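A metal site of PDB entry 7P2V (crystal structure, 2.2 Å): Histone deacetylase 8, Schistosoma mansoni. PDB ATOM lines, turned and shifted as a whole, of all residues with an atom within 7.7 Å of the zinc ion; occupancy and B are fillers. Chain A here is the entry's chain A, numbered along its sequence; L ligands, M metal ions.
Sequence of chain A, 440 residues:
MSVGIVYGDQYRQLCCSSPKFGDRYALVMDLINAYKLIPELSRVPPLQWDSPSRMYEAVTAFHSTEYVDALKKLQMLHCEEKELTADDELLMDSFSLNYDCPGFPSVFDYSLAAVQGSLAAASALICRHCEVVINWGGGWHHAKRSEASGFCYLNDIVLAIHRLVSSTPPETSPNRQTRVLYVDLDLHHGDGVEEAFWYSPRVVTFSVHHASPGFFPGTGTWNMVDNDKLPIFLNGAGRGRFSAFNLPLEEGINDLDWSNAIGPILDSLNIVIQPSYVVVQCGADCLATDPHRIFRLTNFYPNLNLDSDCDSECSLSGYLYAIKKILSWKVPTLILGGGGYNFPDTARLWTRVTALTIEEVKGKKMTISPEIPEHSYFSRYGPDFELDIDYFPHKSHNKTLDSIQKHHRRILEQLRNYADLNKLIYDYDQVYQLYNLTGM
OD2 of Asp 186 sits at hydrogen-bond distance from N of Gly 339, at 3.0 Å. The side-chain carboxylate (OD2) of Asp 186 is in hydrogen-bond range of the side-chain amide nitrogen (NE2) of Gln 281, at 3.1 Å. N of Asp 186 is in hydrogen-bond range of OD1 of Asp 184 (3.1 Å). N of Leu 187 sits at hydrogen-bond distance from OD1 of Asp 285 (2.9 Å).
OD1 of Asp 186 is bound to the zinc ion. The zinc ion is bound by OD2 of Asp 285 (2.0 Å). ND1 of His 188 is bound to the zinc ion. O3 of the ligand is bound to the zinc ion. The zinc ion is bound by an oxygen (O1) of the ligand (2.3 Å).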
ATOM      1  N   PHE A  21      27.218  13.379  30.552  1.00  0.00           N
ATOM      2  CA  PHE A  21      27.124  14.792  30.203  1.00  0.00           C
ATOM      3  C   PHE A  21      27.952  15.687  31.114  1.00  0.00           C
ATOM      4  O   PHE A  21      28.049  16.897  30.838  1.00  0.00           O
ATOM      5  CB  PHE A  21      25.664  15.245  30.194  1.00  0.00           C
ATOM      6  CG  PHE A  21      24.846  14.618  29.101  1.00  0.00           C
ATOM      7  CD1 PHE A  21      24.967  15.075  27.795  1.00  0.00           C
ATOM      8  CD2 PHE A  21      23.973  13.583  29.368  1.00  0.00           C
ATOM      9  CE1 PHE A  21      24.220  14.505  26.776  1.00  0.00           C
ATOM     10  CE2 PHE A  21      23.227  13.004  28.360  1.00  0.00           C
ATOM     11  CZ  PHE A  21      23.346  13.467  27.061  1.00  0.00           C
ATOM     12  N   GLY A 139      14.601  17.159  28.514  1.00  0.00           N
ATOM     13  CA  GLY A 139      14.512  16.683  27.148  1.00  0.00           C
ATOM     14  C   GLY A 139      14.972  15.263  26.905  1.00  0.00           C
ATOM     15  O   GLY A 139      15.415  14.948  25.798  1.00  0.00           O
ATOM     16  N   HIS A 141      14.052  12.323  25.889  1.00  0.00           N
ATOM     17  CA  HIS A 141      12.914  11.784  25.153  1.00  0.00           C
ATOM     18  C   HIS A 141      12.939  10.268  24.964  1.00  0.00           C
ATOM     19  O   HIS A 141      11.934   9.717  24.510  1.00  0.00           O
ATOM     20  CB  HIS A 141      12.807  12.449  23.773  1.00  0.00           C
ATOM     21  CG  HIS A 141      14.066  12.389  22.962  1.00  0.00           C
ATOM     22  ND1 HIS A 141      14.122  12.801  21.655  1.00  0.00           N
ATOM     23  CD2 HIS A 141      15.319  11.968  23.282  1.00  0.00           C
ATOM     24  CE1 HIS A 141      15.356  12.641  21.200  1.00  0.00           C
ATOM     25  NE2 HIS A 141      16.100  12.144  22.169  1.00  0.00           N
ATOM     26  N   HIS A 142      14.030   9.585  25.311  1.00  0.00           N
ATOM     27  CA  HIS A 142      14.099   8.143  25.063  1.00  0.00           C
ATOM     28  C   HIS A 142      13.544   7.307  26.203  1.00  0.00           C
ATOM     29  O   HIS A 142      13.264   6.122  26.001  1.00  0.00           O
ATOM     30  CB  HIS A 142      15.541   7.705  24.785  1.00  0.00           C
ATOM     31  CG  HIS A 142      16.087   8.238  23.497  1.00  0.00           C
ATOM     32  ND1 HIS A 142      15.421   8.118  22.294  1.00  0.00           N
ATOM     33  CD2 HIS A 142      17.234   8.911  23.223  1.00  0.00           C
ATOM     34  CE1 HIS A 142      16.139   8.683  21.342  1.00  0.00           C
ATOM     35  NE2 HIS A 142      17.240   9.173  21.878  1.00  0.00           N
ATOM     36  N   GLY A 150      19.196   5.122  25.829  1.00  0.00           N
ATOM     37  CA  GLY A 150      20.002   6.240  25.367  1.00  0.00           C
ATOM     38  C   GLY A 150      20.327   7.254  26.446  1.00  0.00           C
ATOM     39  O   GLY A 150      20.136   8.460  26.258  1.00  0.00           O
ATOM     40  N   ASP A 184      10.251  17.597  18.048  1.00  0.00           N
ATOM     41  CA  ASP A 184      11.513  16.974  18.465  1.00  0.00           C
ATOM     42  C   ASP A 184      12.572  17.228  17.402  1.00  0.00           C
ATOM     43  O   ASP A 184      12.584  16.558  16.358  1.00  0.00           O
ATOM     44  CB  ASP A 184      11.306  15.478  18.719  1.00  0.00           C
ATOM     45  CG  ASP A 184      12.470  14.838  19.451  1.00  0.00           C
ATOM     46  OD1 ASP A 184      13.632  15.175  19.136  1.00  0.00           O
ATOM     47  OD2 ASP A 184      12.227  13.995  20.338  1.00  0.00           O
ATOM     48  N   LEU A 185      13.482  18.161  17.677  1.00  0.00           N
ATOM     49  CA  LEU A 185      14.529  18.557  16.730  1.00  0.00           C
ATOM     50  C   LEU A 185      15.845  17.813  16.938  1.00  0.00           C
ATOM     51  O   LEU A 185      16.775  18.030  16.160  1.00  0.00           O
ATOM     52  CB  LEU A 185      14.772  20.069  16.834  1.00  0.00           C
ATOM     53  CG  LEU A 185      13.538  20.969  16.792  1.00  0.00           C
ATOM     54  CD1 LEU A 185      13.947  22.421  16.995  1.00  0.00           C
ATOM     55  CD2 LEU A 185      12.790  20.805  15.469  1.00  0.00           C
ATOM     56  N   ASP A 186      15.936  16.963  17.956  1.00  0.00           N
ATOM     57  CA  ASP A 186      17.099  16.121  18.206  1.00  0.00           C
ATOM     58  C   ASP A 186      17.504  15.368  16.947  1.00  0.00           C
ATOM     59  O   ASP A 186      16.674  15.149  16.050  1.00  0.00           O
ATOM     60  CB  ASP A 186      16.791  15.132  19.343  1.00  0.00           C
ATOM     61  CG  ASP A 186      18.043  14.533  19.988  1.00  0.00           C
ATOM     62  OD1 ASP A 186      18.592  13.548  19.435  1.00  0.00           O
ATOM     63  OD2 ASP A 186      18.460  15.031  21.049  1.00  0.00           O
ATOM     64  N   LEU A 187      18.780  14.960  16.852  1.00  0.00           N
ATOM     65  CA  LEU A 187      19.222  14.113  15.748  1.00  0.00           C
ATOM     66  C   LEU A 187      18.598  12.721  15.814  1.00  0.00           C
ATOM     67  O   LEU A 187      18.524  12.042  14.786  1.00  0.00           O
ATOM     68  CB  LEU A 187      20.745  13.982  15.759  1.00  0.00           C
ATOM     69  CG  LEU A 187      21.352  13.002  14.739  1.00  0.00           C
ATOM     70  CD1 LEU A 187      21.332  13.620  13.355  1.00  0.00           C
ATOM     71  CD2 LEU A 187      22.771  12.591  15.118  1.00  0.00           C
ATOM     72  N   HIS A 188      18.162  12.287  16.992  1.00  0.00           N
ATOM     73  CA  HIS A 188      17.603  10.959  17.181  1.00  0.00           C
ATOM     74  C   HIS A 188      16.081  11.022  17.263  1.00  0.00           C
ATOM     75  O   HIS A 188      15.511  12.022  17.712  1.00  0.00           O
ATOM     76  CB  HIS A 188      18.164  10.302  18.455  1.00  0.00           C
ATOM     77  CG  HIS A 188      19.633  10.015  18.391  1.00  0.00           C
ATOM     78  ND1 HIS A 188      20.582  10.871  18.918  1.00  0.00           N
ATOM     79  CD2 HIS A 188      20.318   8.963  17.880  1.00  0.00           C
ATOM     80  CE1 HIS A 188      21.784  10.359  18.722  1.00  0.00           C
ATOM     81  NE2 HIS A 188      21.653   9.211  18.101  1.00  0.00           N
ATOM     82  N   HIS A 189      15.440   9.938  16.834  1.00  0.00           N
ATOM     83  CA  HIS A 189      13.986   9.865  16.894  1.00  0.00           C
ATOM     84  C   HIS A 189      13.518   9.914  18.347  1.00  0.00           C
ATOM     85  O   HIS A 189      14.049   9.197  19.207  1.00  0.00           O
ATOM     86  CB  HIS A 189      13.509   8.571  16.227  1.00  0.00           C
ATOM     87  CG  HIS A 189      12.041   8.305  16.384  1.00  0.00           C
ATOM     88  ND1 HIS A 189      11.546   7.142  16.910  1.00  0.00           N
ATOM     89  CD2 HIS A 189      10.960   9.074  16.084  1.00  0.00           C
ATOM     90  CE1 HIS A 189      10.229   7.183  16.923  1.00  0.00           C
ATOM     91  NE2 HIS A 189       9.850   8.348  16.432  1.00  0.00           N
ATOM     92  N   PHE A 215      21.200   2.426  13.132  1.00  0.00           N
ATOM     93  CA  PHE A 215      21.317   3.712  13.815  1.00  0.00           C
ATOM     94  C   PHE A 215      20.293   3.833  14.936  1.00  0.00           C
ATOM     95  O   PHE A 215      19.110   3.512  14.752  1.00  0.00           O
ATOM     96  CB  PHE A 215      21.158   4.872  12.836  1.00  0.00           C
ATOM     97  CG  PHE A 215      21.318   6.228  13.476  1.00  0.00           C
ATOM     98  CD1 PHE A 215      22.581   6.729  13.789  1.00  0.00           C
ATOM     99  CD2 PHE A 215      20.207   7.007  13.777  1.00  0.00           C
ATOM    100  CE1 PHE A 215      22.737   7.968  14.371  1.00  0.00           C
ATOM    101  CE2 PHE A 215      20.354   8.247  14.371  1.00  0.00           C
ATOM    102  CZ  PHE A 215      21.621   8.734  14.669  1.00  0.00           C
ATOM    103  N   PHE A 216      20.747   4.311  16.095  1.00  0.00           N
ATOM    104  CA  PHE A 216      19.883   4.392  17.265  1.00  0.00           C
ATOM    105  C   PHE A 216      18.787   5.436  17.035  1.00  0.00           C
ATOM    106  O   PHE A 216      19.051   6.494  16.469  1.00  0.00           O
ATOM    107  CB  PHE A 216      20.713   4.767  18.504  1.00  0.00           C
ATOM    108  CG  PHE A 216      19.885   4.932  19.758  1.00  0.00           C
ATOM    109  CD1 PHE A 216      19.519   3.818  20.507  1.00  0.00           C
ATOM    110  CD2 PHE A 216      19.498   6.181  20.196  1.00  0.00           C
ATOM    111  CE1 PHE A 216      18.762   3.954  21.665  1.00  0.00           C
ATOM    112  CE2 PHE A 216      18.741   6.327  21.344  1.00  0.00           C
ATOM    113  CZ  PHE A 216      18.377   5.207  22.087  1.00  0.00           C
ATOM    114  N   GLN A 281      11.693  19.860  21.935  1.00  0.00           N
ATOM    115  CA  GLN A 281      12.965  19.253  22.296  1.00  0.00           C
ATOM    116  C   GLN A 281      14.021  19.745  21.315  1.00  0.00           C
ATOM    117  O   GLN A 281      13.905  19.521  20.109  1.00  0.00           O
ATOM    118  CB  GLN A 281      12.863  17.720  22.261  1.00  0.00           C
ATOM    119  CG  GLN A 281      13.935  16.984  23.063  1.00  0.00           C
ATOM    120  CD  GLN A 281      15.188  16.687  22.252  1.00  0.00           C
ATOM    121  OE1 GLN A 281      15.381  17.237  21.169  1.00  0.00           O
ATOM    122  NE2 GLN A 281      16.034  15.819  22.772  1.00  0.00           N
ATOM    123  N   GLY A 283      17.467  19.155  21.174  1.00  0.00           N
ATOM    124  CA  GLY A 283      18.750  18.468  21.250  1.00  0.00           C
ATOM    125  C   GLY A 283      19.747  18.988  20.241  1.00  0.00           C
ATOM    126  O   GLY A 283      19.371  19.272  19.089  1.00  0.00           O
ATOM    127  N   ALA A 284      21.008  19.104  20.626  1.00  0.00           N
ATOM    128  CA  ALA A 284      22.000  19.804  19.823  1.00  0.00           C
ATOM    129  C   ALA A 284      22.960  18.865  19.104  1.00  0.00           C
ATOM    130  O   ALA A 284      24.044  19.289  18.701  1.00  0.00           O
ATOM    131  CB  ALA A 284      22.788  20.792  20.690  1.00  0.00           C
ATOM    132  N   ASP A 285      22.577  17.602  18.910  1.00  0.00           N
ATOM    133  CA  ASP A 285      23.460  16.688  18.203  1.00  0.00           C
ATOM    134  C   ASP A 285      23.299  16.740  16.694  1.00  0.00           C
ATOM    135  O   ASP A 285      23.906  15.929  15.990  1.00  0.00           O
ATOM    136  CB  ASP A 285      23.264  15.241  18.709  1.00  0.00           C
ATOM    137  CG  ASP A 285      21.817  14.909  19.060  1.00  0.00           C
ATOM    138  OD1 ASP A 285      20.902  15.669  18.698  1.00  0.00           O
ATOM    139  OD2 ASP A 285      21.621  13.869  19.711  1.00  0.00           O
ATOM    140  N   CYS A 286      22.512  17.687  16.170  1.00  0.00           N
ATOM    141  CA  CYS A 286      22.433  17.945  14.736  1.00  0.00           C
ATOM    142  C   CYS A 286      23.523  18.881  14.239  1.00  0.00           C
ATOM    143  O   CYS A 286      23.706  18.994  13.023  1.00  0.00           O
ATOM    144  CB  CYS A 286      21.073  18.526  14.363  1.00  0.00           C
ATOM    145  SG  CYS A 286      19.657  17.413  14.570  1.00  0.00           S
ATOM    146  N   ASP A 290      29.114  18.024  16.066  1.00  0.00           N
ATOM    147  CA  ASP A 290      28.849  16.942  16.993  1.00  0.00           C
ATOM    148  C   ASP A 290      29.716  15.731  16.651  1.00  0.00           C
ATOM    149  O   ASP A 290      30.049  15.508  15.485  1.00  0.00           O
ATOM    150  CB  ASP A 290      27.372  16.564  16.974  1.00  0.00           C
ATOM    151  CG  ASP A 290      26.991  15.634  18.106  1.00  0.00           C
ATOM    152  OD1 ASP A 290      26.663  16.141  19.198  1.00  0.00           O
ATOM    153  OD2 ASP A 290      27.008  14.403  17.895  1.00  0.00           O
ATOM    154  N   HIS A 292      28.912  12.632  16.519  1.00  0.00           N
ATOM    155  CA  HIS A 292      28.197  11.772  15.575  1.00  0.00           C
ATOM    156  C   HIS A 292      28.506  12.164  14.139  1.00  0.00           C
ATOM    157  O   HIS A 292      28.725  11.307  13.284  1.00  0.00           O
ATOM    158  CB  HIS A 292      26.687  11.850  15.814  1.00  0.00           C
ATOM    159  CG  HIS A 292      26.218  11.208  17.086  1.00  0.00           C
ATOM    160  ND1 HIS A 292      26.243  11.857  18.299  1.00  0.00           N
ATOM    161  CD2 HIS A 292      25.680   9.985  17.320  1.00  0.00           C
ATOM    162  CE1 HIS A 292      25.752  11.057  19.237  1.00  0.00           C
ATOM    163  NE2 HIS A 292      25.406   9.916  18.668  1.00  0.00           N
ATOM    164  N   GLY A 338      18.349  18.308  25.478  1.00  0.00           N
ATOM    165  CA  GLY A 338      18.403  16.988  24.870  1.00  0.00           C
ATOM    166  C   GLY A 338      19.838  16.602  24.584  1.00  0.00           C
ATOM    167  O   GLY A 338      20.749  16.938  25.331  1.00  0.00           O
ATOM    168  N   GLY A 339      20.009  15.860  23.495  1.00  0.00           N
ATOM    169  CA  GLY A 339      21.317  15.380  23.111  1.00  0.00           C
ATOM    170  C   GLY A 339      22.291  16.514  22.817  1.00  0.00           C
ATOM    171  O   GLY A 339      21.925  17.681  22.650  1.00  0.00           O
ATOM    172  N   GLY A 340      23.559  16.143  22.741  1.00  0.00           N
ATOM    173  CA  GLY A 340      24.610  17.108  22.459  1.00  0.00           C
ATOM    174  C   GLY A 340      25.860  16.795  23.237  1.00  0.00           C
ATOM    175  O   GLY A 340      25.935  17.060  24.436  1.00  0.00           O
ATOM    176  N   TYR A 341      26.852  16.211  22.566  1.00  0.00           N
ATOM    177  CA  TYR A 341      28.058  15.746  23.240  1.00  0.00           C
ATOM    178  C   TYR A 341      29.264  16.624  22.980  1.00  0.00           C
ATOM    179  O   TYR A 341      30.300  16.430  23.620  1.00  0.00           O
ATOM    180  CB  TYR A 341      28.344  14.297  22.827  1.00  0.00           C
ATOM    181  CG  TYR A 341      27.140  13.401  23.018  1.00  0.00           C
ATOM    182  CD1 TYR A 341      26.099  13.390  22.096  1.00  0.00           C
ATOM    183  CD2 TYR A 341      27.022  12.618  24.160  1.00  0.00           C
ATOM    184  CE1 TYR A 341      24.980  12.595  22.283  1.00  0.00           C
ATOM    185  CE2 TYR A 341      25.903  11.813  24.357  1.00  0.00           C
ATOM    186  CZ  TYR A 341      24.891  11.809  23.421  1.00  0.00           C
ATOM    187  OH  TYR A 341      23.786  11.006  23.619  1.00  0.00           O
HETATM  188  O1  LIG L   1      18.799  12.122  22.045  1.00  0.00           O
HETATM  189  O2  LIG L   1      18.969  11.984  24.216  1.00  0.00           O
HETATM  190  C1  LIG L   1      19.458  11.805  23.074  1.00  0.00           C
HETATM  191  C2  LIG L   1      20.854  11.217  22.928  1.00  0.00           C
HETATM  192  O3  LIG L   1      21.510  11.864  21.882  1.00  0.00           O
HETATM  193  C3  LIG L   1      20.720   9.711  22.649  1.00  0.00           C
HETATM  194  O4  LIG L   1      20.000   9.514  21.463  1.00  0.00           O
HETATM  195  C4  LIG L   1      22.090   9.051  22.523  1.00  0.00           C
HETATM  196  O5  LIG L   1      22.750   9.146  21.457  1.00  0.00           O
HETATM  197  O6  LIG L   1      22.556   8.402  23.498  1.00  0.00           O
HETATM  198 ZN    ZN M   1      20.137  12.691  20.230  1.00  0.00          ZN
